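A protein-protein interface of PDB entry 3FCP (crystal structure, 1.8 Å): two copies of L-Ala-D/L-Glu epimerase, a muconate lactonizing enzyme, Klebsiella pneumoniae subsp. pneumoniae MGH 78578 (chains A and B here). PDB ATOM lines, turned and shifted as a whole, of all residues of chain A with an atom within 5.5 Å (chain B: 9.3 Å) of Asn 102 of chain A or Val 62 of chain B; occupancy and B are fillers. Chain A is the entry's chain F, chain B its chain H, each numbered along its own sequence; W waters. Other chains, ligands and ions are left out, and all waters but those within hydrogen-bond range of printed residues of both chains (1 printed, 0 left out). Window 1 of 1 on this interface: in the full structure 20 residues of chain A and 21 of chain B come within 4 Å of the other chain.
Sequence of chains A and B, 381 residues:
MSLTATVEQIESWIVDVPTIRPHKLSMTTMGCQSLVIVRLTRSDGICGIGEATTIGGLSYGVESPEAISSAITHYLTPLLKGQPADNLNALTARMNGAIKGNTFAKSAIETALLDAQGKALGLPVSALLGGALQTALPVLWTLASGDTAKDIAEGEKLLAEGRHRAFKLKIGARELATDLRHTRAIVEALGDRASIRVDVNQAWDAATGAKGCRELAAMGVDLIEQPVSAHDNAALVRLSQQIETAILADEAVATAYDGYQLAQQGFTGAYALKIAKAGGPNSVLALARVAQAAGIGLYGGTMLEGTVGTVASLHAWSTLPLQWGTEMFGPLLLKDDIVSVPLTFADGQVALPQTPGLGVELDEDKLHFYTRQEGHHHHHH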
ATOM      1  N   VAL A  62      -5.040  -4.224 -13.804  1.00  0.00           N
ATOM      2  CA  VAL A  62      -6.505  -4.171 -13.839  1.00  0.00           C
ATOM      3  C   VAL A  62      -7.056  -3.471 -15.082  1.00  0.00           C
ATOM      4  O   VAL A  62      -8.265  -3.486 -15.328  1.00  0.00           O
ATOM      5  CB  VAL A  62      -7.077  -3.455 -12.584  1.00  0.00           C
ATOM      6  CG1 VAL A  62      -6.497  -4.079 -11.311  1.00  0.00           C
ATOM      7  CG2 VAL A  62      -6.770  -1.959 -12.641  1.00  0.00           C
ATOM      8  N   GLU A  63      -6.172  -2.857 -15.859  1.00  0.00           N
ATOM      9  CA  GLU A  63      -6.578  -2.155 -17.062  1.00  0.00           C
ATOM     10  C   GLU A  63      -6.163  -2.930 -18.317  1.00  0.00           C
ATOM     11  O   GLU A  63      -4.976  -3.146 -18.576  1.00  0.00           O
ATOM     12  CB  GLU A  63      -5.964  -0.745 -17.078  1.00  0.00           C
ATOM     13  CG  GLU A  63      -6.420   0.135 -15.908  1.00  0.00           C
ATOM     14  CD  GLU A  63      -5.753   1.506 -15.885  1.00  0.00           C
ATOM     15  OE1 GLU A  63      -5.745   2.198 -16.924  1.00  0.00           O
ATOM     16  OE2 GLU A  63      -5.253   1.901 -14.812  1.00  0.00           O
ATOM     17  N   ALA A  67     -10.340  -1.957 -22.097  1.00  0.00           N
ATOM     18  CA  ALA A  67     -10.878  -1.092 -21.052  1.00  0.00           C
ATOM     19  C   ALA A  67     -10.207   0.278 -21.194  1.00  0.00           C
ATOM     20  O   ALA A  67     -10.836   1.319 -20.992  1.00  0.00           O
ATOM     21  CB  ALA A  67     -10.605  -1.687 -19.675  1.00  0.00           C
ATOM     22  N   ALA A  71     -12.150   3.795 -21.856  1.00  0.00           N
ATOM     23  CA  ALA A  71     -12.025   4.974 -21.004  1.00  0.00           C
ATOM     24  C   ALA A  71     -11.767   6.212 -21.851  1.00  0.00           C
ATOM     25  O   ALA A  71     -12.327   7.277 -21.598  1.00  0.00           O
ATOM     26  CB  ALA A  71     -10.899   4.785 -20.006  1.00  0.00           C
ATOM     27  N   LEU A  76     -12.794  10.133 -21.301  1.00  0.00           N
ATOM     28  CA  LEU A  76     -11.780  11.171 -21.461  1.00  0.00           C
ATOM     29  C   LEU A  76     -11.984  12.092 -22.656  1.00  0.00           C
ATOM     30  O   LEU A  76     -11.726  13.289 -22.565  1.00  0.00           O
ATOM     31  CB  LEU A  76     -10.386  10.538 -21.540  1.00  0.00           C
ATOM     32  CG  LEU A  76      -9.863  10.003 -20.205  1.00  0.00           C
ATOM     33  CD1 LEU A  76      -8.710   9.035 -20.443  1.00  0.00           C
ATOM     34  CD2 LEU A  76      -9.420  11.164 -19.334  1.00  0.00           C
ATOM     35  N   ILE A  99     -12.233  11.437 -13.370  1.00  0.00           N
ATOM     36  CA  ILE A  99     -11.965  10.030 -13.648  1.00  0.00           C
ATOM     37  C   ILE A  99     -11.093   9.379 -12.579  1.00  0.00           C
ATOM     38  O   ILE A  99      -9.959   9.811 -12.349  1.00  0.00           O
ATOM     39  CB  ILE A  99     -11.233   9.852 -15.007  1.00  0.00           C
ATOM     40  CG1 ILE A  99     -11.970  10.610 -16.119  1.00  0.00           C
ATOM     41  CG2 ILE A  99     -11.111   8.369 -15.343  1.00  0.00           C
ATOM     42  CD1 ILE A  99     -13.411  10.211 -16.310  1.00  0.00           C
ATOM     43  N   LYS A 100     -11.621   8.339 -11.933  1.00  0.00           N
ATOM     44  CA  LYS A 100     -10.883   7.609 -10.908  1.00  0.00           C
ATOM     45  C   LYS A 100     -10.003   6.560 -11.588  1.00  0.00           C
ATOM     46  O   LYS A 100     -10.432   5.903 -12.538  1.00  0.00           O
ATOM     47  CB  LYS A 100     -11.848   6.911  -9.944  1.00  0.00           C
ATOM     48  CG  LYS A 100     -12.694   7.849  -9.094  1.00  0.00           C
ATOM     49  CD  LYS A 100     -11.822   8.716  -8.205  1.00  0.00           C
ATOM     50  CE  LYS A 100     -12.655   9.489  -7.187  1.00  0.00           C
ATOM     51  NZ  LYS A 100     -11.804  10.267  -6.234  1.00  0.00           N
ATOM     52  N   GLY A 101      -8.779   6.398 -11.098  1.00  0.00           N
ATOM     53  CA  GLY A 101      -7.878   5.421 -11.686  1.00  0.00           C
ATOM     54  C   GLY A 101      -7.671   5.608 -13.179  1.00  0.00           C
ATOM     55  O   GLY A 101      -7.506   6.738 -13.652  1.00  0.00           O
ATOM     56  N   ASN A 102      -7.678   4.502 -13.923  1.00  0.00           N
ATOM     57  CA  ASN A 102      -7.480   4.531 -15.376  1.00  0.00           C
ATOM     58  C   ASN A 102      -6.234   5.332 -15.769  1.00  0.00           C
ATOM     59  O   ASN A 102      -6.247   6.116 -16.729  1.00  0.00           O
ATOM     60  CB  ASN A 102      -8.730   5.106 -16.050  1.00  0.00           C
ATOM     61  CG  ASN A 102      -9.924   4.169 -15.939  1.00  0.00           C
ATOM     62  OD1 ASN A 102     -10.156   3.338 -16.818  1.00  0.00           O
ATOM     63  ND2 ASN A 102     -10.670   4.281 -14.843  1.00  0.00           N
ATOM     64  N   THR A 103      -5.156   5.113 -15.019  1.00  0.00           N
ATOM     65  CA  THR A 103      -3.892   5.797 -15.248  1.00  0.00           C
ATOM     66  C   THR A 103      -3.263   5.460 -16.597  1.00  0.00           C
ATOM     67  O   THR A 103      -2.537   6.282 -17.163  1.00  0.00           O
ATOM     68  CB  THR A 103      -2.871   5.486 -14.128  1.00  0.00           C
ATOM     69  OG1 THR A 103      -2.650   4.068 -14.051  1.00  0.00           O
ATOM     70  CG2 THR A 103      -3.391   6.001 -12.786  1.00  0.00           C
ATOM     71  N   PHE A 104      -3.531   4.260 -17.113  1.00  0.00           N
ATOM     72  CA  PHE A 104      -2.971   3.878 -18.406  1.00  0.00           C
ATOM     73  C   PHE A 104      -3.552   4.765 -19.504  1.00  0.00           C
ATOM     74  O   PHE A 104      -2.817   5.267 -20.357  1.00  0.00           O
ATOM     75  CB  PHE A 104      -3.254   2.401 -18.713  1.00  0.00           C
ATOM     76  CG  PHE A 104      -2.293   1.443 -18.044  1.00  0.00           C
ATOM     77  CD1 PHE A 104      -1.508   0.581 -18.807  1.00  0.00           C
ATOM     78  CD2 PHE A 104      -2.182   1.394 -16.655  1.00  0.00           C
ATOM     79  CE1 PHE A 104      -0.628  -0.319 -18.197  1.00  0.00           C
ATOM     80  CE2 PHE A 104      -1.302   0.495 -16.033  1.00  0.00           C
ATOM     81  CZ  PHE A 104      -0.527  -0.359 -16.807  1.00  0.00           C
ATOM     82  N   ALA A 105      -4.870   4.966 -19.475  1.00  0.00           N
ATOM     83  CA  ALA A 105      -5.537   5.815 -20.462  1.00  0.00           C
ATOM     84  C   ALA A 105      -5.074   7.262 -20.323  1.00  0.00           C
ATOM     85  O   ALA A 105      -4.812   7.939 -21.318  1.00  0.00           O
ATOM     86  CB  ALA A 105      -7.050   5.738 -20.292  1.00  0.00           C
ATOM     87  N   LYS A 106      -4.982   7.735 -19.081  1.00  0.00           N
ATOM     88  CA  LYS A 106      -4.548   9.099 -18.828  1.00  0.00           C
ATOM     89  C   LYS A 106      -3.128   9.298 -19.338  1.00  0.00           C
ATOM     90  O   LYS A 106      -2.790  10.357 -19.858  1.00  0.00           O
ATOM     91  CB  LYS A 106      -4.606   9.416 -17.329  1.00  0.00           C
ATOM     92  CG  LYS A 106      -6.019   9.506 -16.763  1.00  0.00           C
ATOM     93  CD  LYS A 106      -6.004   9.675 -15.247  1.00  0.00           C
ATOM     94  CE  LYS A 106      -7.417   9.685 -14.666  1.00  0.00           C
ATOM     95  NZ  LYS A 106      -7.387   9.686 -13.163  1.00  0.00           N
ATOM     96  N   SER A 107      -2.295   8.277 -19.172  1.00  0.00           N
ATOM     97  CA  SER A 107      -0.914   8.345 -19.611  1.00  0.00           C
ATOM     98  C   SER A 107      -0.818   8.555 -21.126  1.00  0.00           C
ATOM     99  O   SER A 107       0.012   9.334 -21.602  1.00  0.00           O
ATOM    100  CB  SER A 107      -0.173   7.069 -19.228  1.00  0.00           C
ATOM    101  OG  SER A 107       1.174   7.165 -19.643  1.00  0.00           O
ATOM    102  N   THR B  54     -22.442   0.657 -11.309  1.00  0.00           N
ATOM    103  CA  THR B  54     -21.697   1.697 -10.631  1.00  0.00           C
ATOM    104  C   THR B  54     -22.448   3.010 -10.741  1.00  0.00           C
ATOM    105  O   THR B  54     -23.565   3.058 -11.257  1.00  0.00           O
ATOM    106  CB  THR B  54     -20.286   1.891 -11.208  1.00  0.00           C
ATOM    107  OG1 THR B  54     -19.570   2.800 -10.362  1.00  0.00           O
ATOM    108  CG2 THR B  54     -20.347   2.461 -12.616  1.00  0.00           C
ATOM    109  N   ILE B  55     -21.816   4.072 -10.258  1.00  0.00           N
ATOM    110  CA  ILE B  55     -22.403   5.402 -10.267  1.00  0.00           C
ATOM    111  C   ILE B  55     -21.513   6.334 -11.081  1.00  0.00           C
ATOM    112  O   ILE B  55     -20.288   6.268 -10.986  1.00  0.00           O
ATOM    113  CB  ILE B  55     -22.510   5.951  -8.812  1.00  0.00           C
ATOM    114  CG1 ILE B  55     -23.331   4.988  -7.950  1.00  0.00           C
ATOM    115  CG2 ILE B  55     -23.146   7.324  -8.807  1.00  0.00           C
ATOM    116  CD1 ILE B  55     -23.168   5.201  -6.440  1.00  0.00           C
ATOM    117  N   GLY B  56     -22.140   7.177 -11.896  1.00  0.00           N
ATOM    118  CA  GLY B  56     -21.422   8.160 -12.693  1.00  0.00           C
ATOM    119  C   GLY B  56     -20.244   7.790 -13.581  1.00  0.00           C
ATOM    120  O   GLY B  56     -19.243   8.515 -13.603  1.00  0.00           O
ATOM    121  N   GLY B  57     -20.355   6.696 -14.326  1.00  0.00           N
ATOM    122  CA  GLY B  57     -19.276   6.303 -15.219  1.00  0.00           C
ATOM    123  C   GLY B  57     -17.984   5.947 -14.511  1.00  0.00           C
ATOM    124  O   GLY B  57     -17.855   4.853 -13.972  1.00  0.00           O
ATOM    125  N   LEU B  58     -17.023   6.868 -14.522  1.00  0.00           N
ATOM    126  CA  LEU B  58     -15.744   6.645 -13.856  1.00  0.00           C
ATOM    127  C   LEU B  58     -15.520   7.696 -12.773  1.00  0.00           C
ATOM    128  O   LEU B  58     -14.410   7.853 -12.268  1.00  0.00           O
ATOM    129  CB  LEU B  58     -14.595   6.693 -14.873  1.00  0.00           C
ATOM    130  CG  LEU B  58     -14.521   5.548 -15.898  1.00  0.00           C
ATOM    131  CD1 LEU B  58     -13.481   5.874 -16.953  1.00  0.00           C
ATOM    132  CD2 LEU B  58     -14.184   4.231 -15.202  1.00  0.00           C
ATOM    133  N   SER B  59     -16.577   8.409 -12.406  1.00  0.00           N
ATOM    134  CA  SER B  59     -16.458   9.459 -11.399  1.00  0.00           C
ATOM    135  C   SER B  59     -16.417   8.973  -9.953  1.00  0.00           C
ATOM    136  O   SER B  59     -15.957   9.695  -9.068  1.00  0.00           O
ATOM    137  CB  SER B  59     -17.591  10.476 -11.564  1.00  0.00           C
ATOM    138  OG  SER B  59     -17.484  11.129 -12.817  1.00  0.00           O
ATOM    139  N   TYR B  60     -16.887   7.757  -9.710  1.00  0.00           N
ATOM    140  CA  TYR B  60     -16.889   7.223  -8.354  1.00  0.00           C
ATOM    141  C   TYR B  60     -15.940   6.054  -8.156  1.00  0.00           C
ATOM    142  O   TYR B  60     -15.335   5.920  -7.095  1.00  0.00           O
ATOM    143  CB  TYR B  60     -18.317   6.843  -7.959  1.00  0.00           C
ATOM    144  CG  TYR B  60     -19.190   8.068  -7.849  1.00  0.00           C
ATOM    145  CD1 TYR B  60     -19.304   8.763  -6.644  1.00  0.00           C
ATOM    146  CD2 TYR B  60     -19.823   8.593  -8.974  1.00  0.00           C
ATOM    147  CE1 TYR B  60     -20.024   9.957  -6.566  1.00  0.00           C
ATOM    148  CE2 TYR B  60     -20.542   9.784  -8.910  1.00  0.00           C
ATOM    149  CZ  TYR B  60     -20.636  10.462  -7.706  1.00  0.00           C
ATOM    150  OH  TYR B  60     -21.329  11.649  -7.654  1.00  0.00           O
ATOM    151  N   GLY B  61     -15.801   5.225  -9.186  1.00  0.00           N
ATOM    152  CA  GLY B  61     -14.914   4.075  -9.112  1.00  0.00           C
ATOM    153  C   GLY B  61     -14.120   3.948 -10.397  1.00  0.00           C
ATOM    154  O   GLY B  61     -14.416   4.635 -11.370  1.00  0.00           O
ATOM    155  N   VAL B  62     -13.128   3.065 -10.415  1.00  0.00           N
ATOM    156  CA  VAL B  62     -12.288   2.889 -11.597  1.00  0.00           C
ATOM    157  C   VAL B  62     -12.872   1.954 -12.660  1.00  0.00           C
ATOM    158  O   VAL B  62     -12.303   1.813 -13.744  1.00  0.00           O
ATOM    159  CB  VAL B  62     -10.887   2.368 -11.202  1.00  0.00           C
ATOM    160  CG1 VAL B  62     -10.316   3.221 -10.073  1.00  0.00           C
ATOM    161  CG2 VAL B  62     -10.970   0.906 -10.789  1.00  0.00           C
ATOM    162  N   GLU B  63     -14.002   1.324 -12.347  1.00  0.00           N
ATOM    163  CA  GLU B  63     -14.659   0.395 -13.267  1.00  0.00           C
ATOM    164  C   GLU B  63     -15.962   0.965 -13.821  1.00  0.00           C
ATOM    165  O   GLU B  63     -16.930   1.160 -13.082  1.00  0.00           O
ATOM    166  CB  GLU B  63     -14.948  -0.929 -12.554  1.00  0.00           C
ATOM    167  CG  GLU B  63     -13.691  -1.673 -12.105  1.00  0.00           C
ATOM    168  CD  GLU B  63     -14.001  -2.989 -11.406  1.00  0.00           C
ATOM    169  OE1 GLU B  63     -14.689  -3.840 -12.005  1.00  0.00           O
ATOM    170  OE2 GLU B  63     -13.545  -3.175 -10.261  1.00  0.00           O
ATOM    171  N   SER B  64     -15.982   1.232 -15.125  1.00  0.00           N
ATOM    172  CA  SER B  64     -17.170   1.778 -15.781  1.00  0.00           C
ATOM    173  C   SER B  64     -18.058   0.651 -16.311  1.00  0.00           C
ATOM    174  O   SER B  64     -17.631  -0.500 -16.402  1.00  0.00           O
ATOM    175  CB  SER B  64     -16.763   2.671 -16.953  1.00  0.00           C
ATOM    176  OG  SER B  64     -16.178   1.898 -17.989  1.00  0.00           O
ATOM    177  N   PRO B  65     -19.311   0.970 -16.668  1.00  0.00           N
ATOM    178  CA  PRO B  65     -20.193  -0.078 -17.189  1.00  0.00           C
ATOM    179  C   PRO B  65     -19.609  -0.725 -18.448  1.00  0.00           C
ATOM    180  O   PRO B  65     -19.699  -1.936 -18.623  1.00  0.00           O
ATOM    181  CB  PRO B  65     -21.497   0.671 -17.465  1.00  0.00           C
ATOM    182  CG  PRO B  65     -21.497   1.736 -16.405  1.00  0.00           C
ATOM    183  CD  PRO B  65     -20.057   2.224 -16.448  1.00  0.00           C
ATOM    184  N   GLU B  66     -19.006   0.073 -19.329  1.00  0.00           N
ATOM    185  CA  GLU B  66     -18.440  -0.507 -20.537  1.00  0.00           C
ATOM    186  C   GLU B  66     -17.178  -1.326 -20.256  1.00  0.00           C
ATOM    187  O   GLU B  66     -16.921  -2.326 -20.927  1.00  0.00           O
ATOM    188  CB  GLU B  66     -18.168   0.571 -21.606  1.00  0.00           C
ATOM    189  CG  GLU B  66     -17.919   1.974 -21.090  1.00  0.00           C
ATOM    190  CD  GLU B  66     -19.173   2.628 -20.533  1.00  0.00           C
ATOM    191  OE1 GLU B  66     -19.214   2.880 -19.318  1.00  0.00           O
ATOM    192  OE2 GLU B  66     -20.116   2.888 -21.309  1.00  0.00           O
ATOM    193  N   ALA B  67     -16.398  -0.923 -19.260  1.00  0.00           N
ATOM    194  CA  ALA B  67     -15.186  -1.666 -18.919  1.00  0.00           C
ATOM    195  C   ALA B  67     -15.575  -2.989 -18.249  1.00  0.00           C
ATOM    196  O   ALA B  67     -14.919  -4.016 -18.444  1.00  0.00           O
ATOM    197  CB  ALA B  67     -14.305  -0.841 -17.991  1.00  0.00           C
ATOM    198  N   ILE B  68     -16.641  -2.946 -17.456  1.00  0.00           N
ATOM    199  CA  ILE B  68     -17.152  -4.129 -16.771  1.00  0.00           C
ATOM    200  C   ILE B  68     -17.641  -5.112 -17.836  1.00  0.00           C
ATOM    201  O   ILE B  68     -17.292  -6.296 -17.822  1.00  0.00           O
ATOM    202  CB  ILE B  68     -18.309  -3.744 -15.823  1.00  0.00           C
ATOM    203  CG1 ILE B  68     -17.742  -2.965 -14.628  1.00  0.00           C
ATOM    204  CG2 ILE B  68     -19.067  -4.996 -15.360  1.00  0.00           C
ATOM    205  CD1 ILE B  68     -18.795  -2.336 -13.742  1.00  0.00           C
ATOM    206  N   LYS B 100      -6.672  -9.516 -12.598  1.00  0.00           N
ATOM    207  CA  LYS B 100      -6.358  -8.586 -11.516  1.00  0.00           C
ATOM    208  C   LYS B 100      -7.522  -7.618 -11.359  1.00  0.00           C
ATOM    209  O   LYS B 100      -8.104  -7.181 -12.352  1.00  0.00           O
ATOM    210  CB  LYS B 100      -5.094  -7.781 -11.842  1.00  0.00           C
ATOM    211  CG  LYS B 100      -3.824  -8.603 -11.985  1.00  0.00           C
ATOM    212  CD  LYS B 100      -3.418  -9.274 -10.681  1.00  0.00           C
ATOM    213  CE  LYS B 100      -2.033  -9.900 -10.812  1.00  0.00           C
ATOM    214  NZ  LYS B 100      -1.612 -10.626  -9.586  1.00  0.00           N
ATOM    215  N   GLY B 101      -7.855  -7.285 -10.117  1.00  0.00           N
ATOM    216  CA  GLY B 101      -8.941  -6.357  -9.863  1.00  0.00           C
ATOM    217  C   GLY B 101     -10.223  -6.716 -10.593  1.00  0.00           C
ATOM    218  O   GLY B 101     -10.619  -7.885 -10.616  1.00  0.00           O
ATOM    219  N   ASN B 102     -10.872  -5.716 -11.190  1.00  0.00           N
ATOM    220  CA  ASN B 102     -12.128  -5.932 -11.912  1.00  0.00           C
ATOM    221  C   ASN B 102     -13.136  -6.651 -11.021  1.00  0.00           C
ATOM    222  O   ASN B 102     -13.823  -7.580 -11.452  1.00  0.00           O
ATOM    223  CB  ASN B 102     -11.871  -6.742 -13.180  1.00  0.00           C
ATOM    224  CG  ASN B 102     -11.163  -5.930 -14.250  1.00  0.00           C
ATOM    225  OD1 ASN B 102     -11.806  -5.327 -15.113  1.00  0.00           O
ATOM    226  ND2 ASN B 102      -9.834  -5.893 -14.191  1.00  0.00           N
ATOM    227  N   THR B 103     -13.221  -6.203  -9.773  1.00  0.00           N
ATOM    228  CA  THR B 103     -14.134  -6.802  -8.811  1.00  0.00           C
ATOM    229  C   THR B 103     -15.608  -6.628  -9.180  1.00  0.00           C
ATOM    230  O   THR B 103     -16.430  -7.474  -8.844  1.00  0.00           O
ATOM    231  CB  THR B 103     -13.908  -6.226  -7.402  1.00  0.00           C
ATOM    232  OG1 THR B 103     -14.135  -4.811  -7.421  1.00  0.00           O
ATOM    233  CG2 THR B 103     -12.476  -6.521  -6.933  1.00  0.00           C
ATOM    234  N   PHE B 104     -15.954  -5.536  -9.858  1.00  0.00           N
ATOM    235  CA  PHE B 104     -17.352  -5.339 -10.239  1.00  0.00           C
ATOM    236  C   PHE B 104     -17.786  -6.470 -11.181  1.00  0.00           C
ATOM    237  O   PHE B 104     -18.836  -7.093 -10.983  1.00  0.00           O
ATOM    238  CB  PHE B 104     -17.551  -3.969 -10.909  1.00  0.00           C
ATOM    239  CG  PHE B 104     -17.681  -2.822  -9.932  1.00  0.00           C
ATOM    240  CD1 PHE B 104     -18.831  -2.028  -9.919  1.00  0.00           C
ATOM    241  CD2 PHE B 104     -16.666  -2.540  -9.021  1.00  0.00           C
ATOM    242  CE1 PHE B 104     -18.967  -0.972  -9.013  1.00  0.00           C
ATOM    243  CE2 PHE B 104     -16.786  -1.485  -8.104  1.00  0.00           C
ATOM    244  CZ  PHE B 104     -17.939  -0.697  -8.099  1.00  0.00           C
ATOM    245  N   GLN B 202     -15.307  11.054   0.372  1.00  0.00           N
ATOM    246  CA  GLN B 202     -13.938  11.493   0.070  1.00  0.00           C
ATOM    247  C   GLN B 202     -13.702  12.978  -0.177  1.00  0.00           C
ATOM    248  O   GLN B 202     -12.569  13.381  -0.425  1.00  0.00           O
ATOM    249  CB  GLN B 202     -13.408  10.754  -1.161  1.00  0.00           C
ATOM    250  CG  GLN B 202     -13.268   9.262  -1.008  1.00  0.00           C
ATOM    251  CD  GLN B 202     -12.641   8.632  -2.238  1.00  0.00           C
ATOM    252  OE1 GLN B 202     -13.326   8.317  -3.217  1.00  0.00           O
ATOM    253  NE2 GLN B 202     -11.327   8.463  -2.201  1.00  0.00           N
ATOM    254  N   HIS B 231      -6.960   8.243  -0.649  1.00  0.00           N
ATOM    255  CA  HIS B 231      -5.532   8.476  -0.883  1.00  0.00           C
ATOM    256  C   HIS B 231      -4.876   8.804   0.462  1.00  0.00           C
ATOM    257  O   HIS B 231      -3.654   8.872   0.568  1.00  0.00           O
ATOM    258  CB  HIS B 231      -5.323   9.676  -1.812  1.00  0.00           C
ATOM    259  CG  HIS B 231      -5.621   9.403  -3.253  1.00  0.00           C
ATOM    260  ND1 HIS B 231      -6.016  10.392  -4.127  1.00  0.00           N
ATOM    261  CD2 HIS B 231      -5.551   8.262  -3.980  1.00  0.00           C
ATOM    262  CE1 HIS B 231      -6.178   9.874  -5.331  1.00  0.00           C
ATOM    263  NE2 HIS B 231      -5.902   8.583  -5.269  1.00  0.00           N
ATOM    264  N   GLU B 251     -14.668   3.841   0.424  1.00  0.00           N
ATOM    265  CA  GLU B 251     -13.642   3.712  -0.608  1.00  0.00           C
ATOM    266  C   GLU B 251     -12.298   3.213  -0.068  1.00  0.00           C
ATOM    267  O   GLU B 251     -11.519   2.606  -0.803  1.00  0.00           O
ATOM    268  CB  GLU B 251     -13.431   5.048  -1.323  1.00  0.00           C
ATOM    269  CG  GLU B 251     -14.452   5.377  -2.416  1.00  0.00           C
ATOM    270  CD  GLU B 251     -15.844   5.671  -1.880  1.00  0.00           C
ATOM    271  OE1 GLU B 251     -15.965   6.132  -0.722  1.00  0.00           O
ATOM    272  OE2 GLU B 251     -16.816   5.453  -2.633  1.00  0.00           O
ATOM    273  N   ALA B 276     -19.734  -5.398  -4.949  1.00  0.00           N
ATOM    274  CA  ALA B 276     -19.002  -4.894  -6.112  1.00  0.00           C
ATOM    275  C   ALA B 276     -17.536  -4.609  -5.803  1.00  0.00           C
ATOM    276  O   ALA B 276     -16.670  -4.807  -6.658  1.00  0.00           O
ATOM    277  CB  ALA B 276     -19.658  -3.628  -6.649  1.00  0.00           C
ATOM    278  N   LYS B 277     -17.254  -4.125  -4.595  1.00  0.00           N
ATOM    279  CA  LYS B 277     -15.870  -3.815  -4.218  1.00  0.00           C
ATOM    280  C   LYS B 277     -15.068  -5.073  -3.903  1.00  0.00           C
ATOM    281  O   LYS B 277     -13.864  -5.119  -4.149  1.00  0.00           O
ATOM    282  CB  LYS B 277     -15.821  -2.893  -2.986  1.00  0.00           C
ATOM    283  CG  LYS B 277     -16.331  -1.468  -3.218  1.00  0.00           C
ATOM    284  CD  LYS B 277     -16.073  -0.568  -2.008  1.00  0.00           C
ATOM    285  CE  LYS B 277     -16.743  -1.086  -0.733  1.00  0.00           C
ATOM    286  NZ  LYS B 277     -16.444  -0.226   0.460  1.00  0.00           N
ATOM    287  N   MET B 303     -24.132   0.182  -4.476  1.00  0.00           N
ATOM    288  CA  MET B 303     -23.592   1.004  -5.554  1.00  0.00           C
ATOM    289  C   MET B 303     -24.808   1.438  -6.367  1.00  0.00           C
ATOM    290  O   MET B 303     -24.706   1.868  -7.520  1.00  0.00           O
ATOM    291  CB  MET B 303     -22.606   0.202  -6.409  1.00  0.00           C
ATOM    292  CG  MET B 303     -21.314  -0.153  -5.664  1.00  0.00           C
ATOM    293  SD  MET B 303     -20.184   1.236  -5.332  1.00  0.00           S
ATOM    294  CE  MET B 303     -21.117   2.308  -4.393  1.00  0.00           C
HETATM  295  O   HOH W   1     -14.366   2.895 -19.371  1.00  0.00           O
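ND2 of Asn 102 of chain B sits at hydrogen-bond distance from O of Val 62 of chain A (3.1 Å).
N of Lys 100 of chain A is in hydrogen-bond range of O of Leu 58 of chain B, at 2.9 Å.
The backbone carbonyl oxygen of Val 62 of chain B lies within hydrogen-bond range of the side-chain amide nitrogen of Asn 102 of chain A (3.2 Å).
The side-chain amino group (NZ) of Lys 106 of chain A lies within hydrogen-bond range of the backbone carbonyl oxygen (O) of Ile 99 of chain A (2.7 Å).
ND2 of Asn 102 of chain A lies within hydrogen-bond range of O of Lys 100 of chain A (2.8 Å).
The backbone carbonyl oxygen (O) of Gly 101 of chain A lies within hydrogen-bond range of the side-chain amino group (NZ) of Lys 106 of chain A, at 3.0 Å.
ND2 of Asn 102 of chain B lies within hydrogen-bond range of O of Lys 100 of chain B, 2.8 Å away.
Among the printed residues, pairs that only touch across the chains: Asn 102 of chain A with Leu 58 of chain B, Ile 99 of chain A with Leu 58 of chain B, Val 62 of chain A with Gly 101 of chain B, Lys 100 of chain A with Val 62 of chain B, Val 62 of chain A with Lys 100 of chain B, Gly 101 of chain A with Val 62 of chain B, Lys 100 of chain A with Gly 61 of chain B, Lys 100 of chain A with Ser 59 of chain B, Lys 100 of chain A with Tyr 60 of chain B and Lys 100 of chain A with Gln 202 of chain B.
Of chain B, only Leu 58 (3.5 Å) and Val 62 (3.2 Å) come within 4 Å of Asn 102 of chain A.
Val 62 of chain B touches three residues of chain A.
Gly 101 of chain A touches one residue of chain B.
No residue of chain B comes within 4 Å of Ala 105 of chain A.
Of the printed residues of chain A, Ser 59 of chain B touches Lys 100 (3.7 Å).
Of the printed residues of chain A, Leu 58 of chain B touches Ile 99 (3.6 Å), Lys 100 (2.9 Å) and Asn 102 (3.5 Å).
Of the printed residues of chain A, Tyr 60 of chain B touches Lys 100.
Of the printed residues of chain B, Lys 100 of chain A touches Leu 58, Ser 59, Tyr 60, Gly 61, Val 62 and Gln 202.
Ser 64 of chain B touches none of the printed residues of chain A.
The nearest residue of chain A that does not touch Val 62 of chain B is Val 62 of chain A (5.4 Å).
The nearest printed residue of chain A that does not touch Gly 101 of chain B is Glu 63 of chain A (7.4 Å).
Of the 14 printed residues of chain A, 5 touch a printed residue of chain B.
Hydrophobic or aromatic side chains of chain A that line the printed part of chain B: Val 62 and Ile 99.
Hydrophobic or aromatic side chains of chain B that line the printed part of chain A: Leu 58 and Val 62.
Among the printed residues, no Asp or Glu carboxylate lies within 4 Å of a Lys or Arg side-chain nitrogen of the other chain.
Val 62 of chain A touches Lys 100 of chain B, and with the chains exchanged Lys 100 of chain A touches Val 62 of chain B.
Val 62 of chain A touches Asn 102 of chain B, and with the chains exchanged Asn 102 of chain A touches Val 62 of chain B.
Positions printed for both chains: 62, 63, 67, 100, 101, 102, 103 and 104.
Of the 13 pairs that touch across the chains among the printed residues, 6 have their exchanged pair printed and touching as well.
Water W1 lies within hydrogen-bond range of the side-chain hydroxyl (OG) of Ser 64 of chain B (2.5 Å) and the backbone NH (N) of Ala 71 of chain A (3.4 Å).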
